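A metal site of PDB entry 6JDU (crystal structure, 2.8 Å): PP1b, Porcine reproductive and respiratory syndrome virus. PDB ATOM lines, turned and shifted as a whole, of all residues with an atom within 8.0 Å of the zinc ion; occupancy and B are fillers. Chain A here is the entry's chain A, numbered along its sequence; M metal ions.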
ATOM      1  N   ILE A  39      13.595  17.928 -23.776  1.00  0.00           N
ATOM      2  CA  ILE A  39      13.221  16.533 -24.024  1.00  0.00           C
ATOM      3  C   ILE A  39      12.040  16.095 -23.157  1.00  0.00           C
ATOM      4  O   ILE A  39      11.587  16.824 -22.279  1.00  0.00           O
ATOM      5  CB  ILE A  39      14.422  15.553 -23.850  1.00  0.00           C
ATOM      6  CG1 ILE A  39      15.032  15.637 -22.449  1.00  0.00           C
ATOM      7  CG2 ILE A  39      15.487  15.831 -24.900  1.00  0.00           C
ATOM      8  CD1 ILE A  39      15.952  14.476 -22.128  1.00  0.00           C
ATOM      9  N   TRP A  40      11.545  14.889 -23.449  1.00  0.00           N
ATOM     10  CA  TRP A  40      10.487  14.195 -22.700  1.00  0.00           C
ATOM     11  C   TRP A  40      10.349  14.480 -21.181  1.00  0.00           C
ATOM     12  O   TRP A  40       9.226  14.569 -20.682  1.00  0.00           O
ATOM     13  CB  TRP A  40      10.540  12.673 -22.984  1.00  0.00           C
ATOM     14  CG  TRP A  40      11.884  11.989 -22.820  1.00  0.00           C
ATOM     15  CD1 TRP A  40      12.332  11.332 -21.716  1.00  0.00           C
ATOM     16  CD2 TRP A  40      12.929  11.862 -23.809  1.00  0.00           C
ATOM     17  NE1 TRP A  40      13.582  10.824 -21.936  1.00  0.00           N
ATOM     18  CE2 TRP A  40      13.983  11.128 -23.217  1.00  0.00           C
ATOM     19  CE3 TRP A  40      13.092  12.301 -25.141  1.00  0.00           C
ATOM     20  CZ2 TRP A  40      15.173  10.819 -23.888  1.00  0.00           C
ATOM     21  CZ3 TRP A  40      14.281  12.005 -25.814  1.00  0.00           C
ATOM     22  CH2 TRP A  40      15.303  11.266 -25.180  1.00  0.00           C
ATOM     23  N   CYS A  41      11.457  14.620 -20.452  1.00  0.00           N
ATOM     24  CA  CYS A  41      11.388  14.926 -19.007  1.00  0.00           C
ATOM     25  C   CYS A  41      11.063  16.386 -18.672  1.00  0.00           C
ATOM     26  O   CYS A  41      10.816  16.704 -17.503  1.00  0.00           O
ATOM     27  CB  CYS A  41      12.681  14.512 -18.289  1.00  0.00           C
ATOM     28  SG  CYS A  41      14.046  15.674 -18.447  1.00  0.00           S
ATOM     29  N   GLY A  42      11.063  17.267 -19.663  1.00  0.00           N
ATOM     30  CA  GLY A  42      10.690  18.678 -19.482  1.00  0.00           C
ATOM     31  C   GLY A  42      11.860  19.622 -19.216  1.00  0.00           C
ATOM     32  O   GLY A  42      11.652  20.841 -19.115  1.00  0.00           O
ATOM     33  N   HIS A  43      13.067  19.079 -19.127  1.00  0.00           N
ATOM     34  CA  HIS A  43      14.293  19.853 -18.958  1.00  0.00           C
ATOM     35  C   HIS A  43      15.163  19.732 -20.211  1.00  0.00           C
ATOM     36  O   HIS A  43      14.831  18.934 -21.110  1.00  0.00           O
ATOM     37  CB  HIS A  43      15.071  19.337 -17.743  1.00  0.00           C
ATOM     38  CG  HIS A  43      14.211  19.087 -16.545  1.00  0.00           C
ATOM     39  ND1 HIS A  43      13.983  17.825 -16.051  1.00  0.00           N
ATOM     40  CD2 HIS A  43      13.545  19.946 -15.739  1.00  0.00           C
ATOM     41  CE1 HIS A  43      13.201  17.915 -14.987  1.00  0.00           C
ATOM     42  NE2 HIS A  43      12.920  19.193 -14.774  1.00  0.00           N
ATOM     43  N   PRO A  44      16.257  20.512 -20.298  1.00  0.00           N
ATOM     44  CA  PRO A  44      17.173  20.340 -21.433  1.00  0.00           C
ATOM     45  C   PRO A  44      17.990  19.058 -21.352  1.00  0.00           C
ATOM     46  O   PRO A  44      18.421  18.656 -20.273  1.00  0.00           O
ATOM     47  CB  PRO A  44      18.110  21.547 -21.340  1.00  0.00           C
ATOM     48  CG  PRO A  44      17.412  22.519 -20.471  1.00  0.00           C
ATOM     49  CD  PRO A  44      16.616  21.706 -19.510  1.00  0.00           C
ATOM     50  N   ALA A  45      18.207  18.421 -22.503  1.00  0.00           N
ATOM     51  CA  ALA A  45      19.050  17.245 -22.587  1.00  0.00           C
ATOM     52  C   ALA A  45      20.429  17.532 -21.992  1.00  0.00           C
ATOM     53  O   ALA A  45      21.032  18.584 -22.276  1.00  0.00           O
ATOM     54  CB  ALA A  45      19.184  16.799 -24.042  1.00  0.00           C
ATOM     55  N   GLY A  46      20.911  16.618 -21.144  1.00  0.00           N
ATOM     56  CA  GLY A  46      22.221  16.727 -20.510  1.00  0.00           C
ATOM     57  C   GLY A  46      22.324  17.701 -19.356  1.00  0.00           C
ATOM     58  O   GLY A  46      23.416  17.924 -18.838  1.00  0.00           O
ATOM     59  N   SER A  47      21.196  18.274 -18.921  1.00  0.00           N
ATOM     60  CA  SER A  47      21.197  19.309 -17.878  1.00  0.00           C
ATOM     61  C   SER A  47      21.398  18.752 -16.468  1.00  0.00           C
ATOM     62  O   SER A  47      21.907  19.461 -15.597  1.00  0.00           O
ATOM     63  CB  SER A  47      19.913  20.153 -17.948  1.00  0.00           C
ATOM     64  OG  SER A  47      18.761  19.372 -17.720  1.00  0.00           O
ATOM     65  N   GLY A  48      21.009  17.501 -16.253  1.00  0.00           N
ATOM     66  CA  GLY A  48      21.051  16.889 -14.933  1.00  0.00           C
ATOM     67  C   GLY A  48      19.992  17.434 -13.977  1.00  0.00           C
ATOM     68  O   GLY A  48      20.152  17.311 -12.759  1.00  0.00           O
ATOM     69  N   SER A  49      18.926  18.018 -14.523  1.00  0.00           N
ATOM     70  CA  SER A  49      17.850  18.609 -13.716  1.00  0.00           C
ATOM     71  C   SER A  49      16.985  17.547 -13.056  1.00  0.00           C
ATOM     72  O   SER A  49      16.440  17.757 -11.970  1.00  0.00           O
ATOM     73  CB  SER A  49      16.969  19.499 -14.596  1.00  0.00           C
ATOM     74  OG  SER A  49      17.739  20.495 -15.239  1.00  0.00           O
ATOM     75  N   CYS A  50      16.829  16.423 -13.750  1.00  0.00           N
ATOM     76  CA  CYS A  50      16.272  15.201 -13.170  1.00  0.00           C
ATOM     77  C   CYS A  50      17.110  14.006 -13.628  1.00  0.00           C
ATOM     78  O   CYS A  50      18.006  14.164 -14.460  1.00  0.00           O
ATOM     79  CB  CYS A  50      14.812  15.026 -13.600  1.00  0.00           C
ATOM     80  SG  CYS A  50      14.563  14.733 -15.370  1.00  0.00           S
ATOM     81  N   SER A  51      16.807  12.833 -13.094  1.00  0.00           N
ATOM     82  CA  SER A  51      17.576  11.620 -13.422  1.00  0.00           C
ATOM     83  C   SER A  51      17.441  11.165 -14.891  1.00  0.00           C
ATOM     84  O   SER A  51      18.300  10.441 -15.399  1.00  0.00           O
ATOM     85  CB  SER A  51      17.239  10.478 -12.456  1.00  0.00           C
ATOM     86  OG  SER A  51      15.843  10.344 -12.271  1.00  0.00           O
ATOM     87  N   GLU A  52      16.380  11.617 -15.563  1.00  0.00           N
ATOM     88  CA  GLU A  52      16.172  11.344 -16.988  1.00  0.00           C
ATOM     89  C   GLU A  52      17.089  12.161 -17.909  1.00  0.00           C
ATOM     90  O   GLU A  52      17.457  11.685 -18.983  1.00  0.00           O
ATOM     91  CB  GLU A  52      14.706  11.618 -17.366  1.00  0.00           C
ATOM     92  CG  GLU A  52      14.266  11.031 -18.695  1.00  0.00           C
ATOM     93  CD  GLU A  52      14.414   9.518 -18.764  1.00  0.00           C
ATOM     94  OE1 GLU A  52      14.201   8.853 -17.729  1.00  0.00           O
ATOM     95  OE2 GLU A  52      14.742   8.998 -19.847  1.00  0.00           O
ATOM     96  N   CYS A  53      17.433  13.386 -17.497  1.00  0.00           N
ATOM     97  CA  CYS A  53      18.342  14.263 -18.257  1.00  0.00           C
ATOM     98  C   CYS A  53      19.793  14.248 -17.727  1.00  0.00           C
ATOM     99  O   CYS A  53      20.580  15.141 -18.066  1.00  0.00           O
ATOM    100  CB  CYS A  53      17.763  15.692 -18.321  1.00  0.00           C
ATOM    101  SG  CYS A  53      17.259  16.430 -16.748  1.00  0.00           S
ATOM    102  N   GLU A  54      20.147  13.262 -16.896  1.00  0.00           N
ATOM    103  CA  GLU A  54      21.530  13.064 -16.436  1.00  0.00           C
ATOM    104  C   GLU A  54      22.512  12.630 -17.535  1.00  0.00           C
ATOM    105  O   GLU A  54      23.641  13.132 -17.564  1.00  0.00           O
ATOM    106  CB  GLU A  54      21.603  12.064 -15.258  1.00  0.00           C
ATOM    107  CG  GLU A  54      21.199  12.629 -13.907  1.00  0.00           C
HETATM  108 ZN    ZN M   1      15.102  16.231 -16.641  1.00  0.00          ZN
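The zinc ion is bound by ND1 of His 43 (2.0 Å). SG of Cys 50 binds the zinc ion, at 2.0 Å. SG of Cys 41 binds the zinc ion (2.2 Å). SG of Cys 53 is bound to the zinc ion, at 2.2 Å. The zinc ion has four donor atoms within binding distance.
The backbone NH of Ser 47 sits at hydrogen-bond distance from the backbone carbonyl oxygen of Cys 53 (3.3 Å). The backbone carbonyl oxygen (O) of Cys 53 sits at hydrogen-bond distance from the backbone NH (N) of Gly 48 (3.0 Å). The side-chain sulfur (SG) of Cys 50 sits close to the backbone NH (N) of Glu 52. The backbone NH (N) of Gly 46 lies close to the backbone carbonyl oxygen (O) of Cys 53 (3.4 Å). The backbone NH (N) of Ser 49 lies close to the side-chain sulfur (SG) of Cys 53 (3.2 Å).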
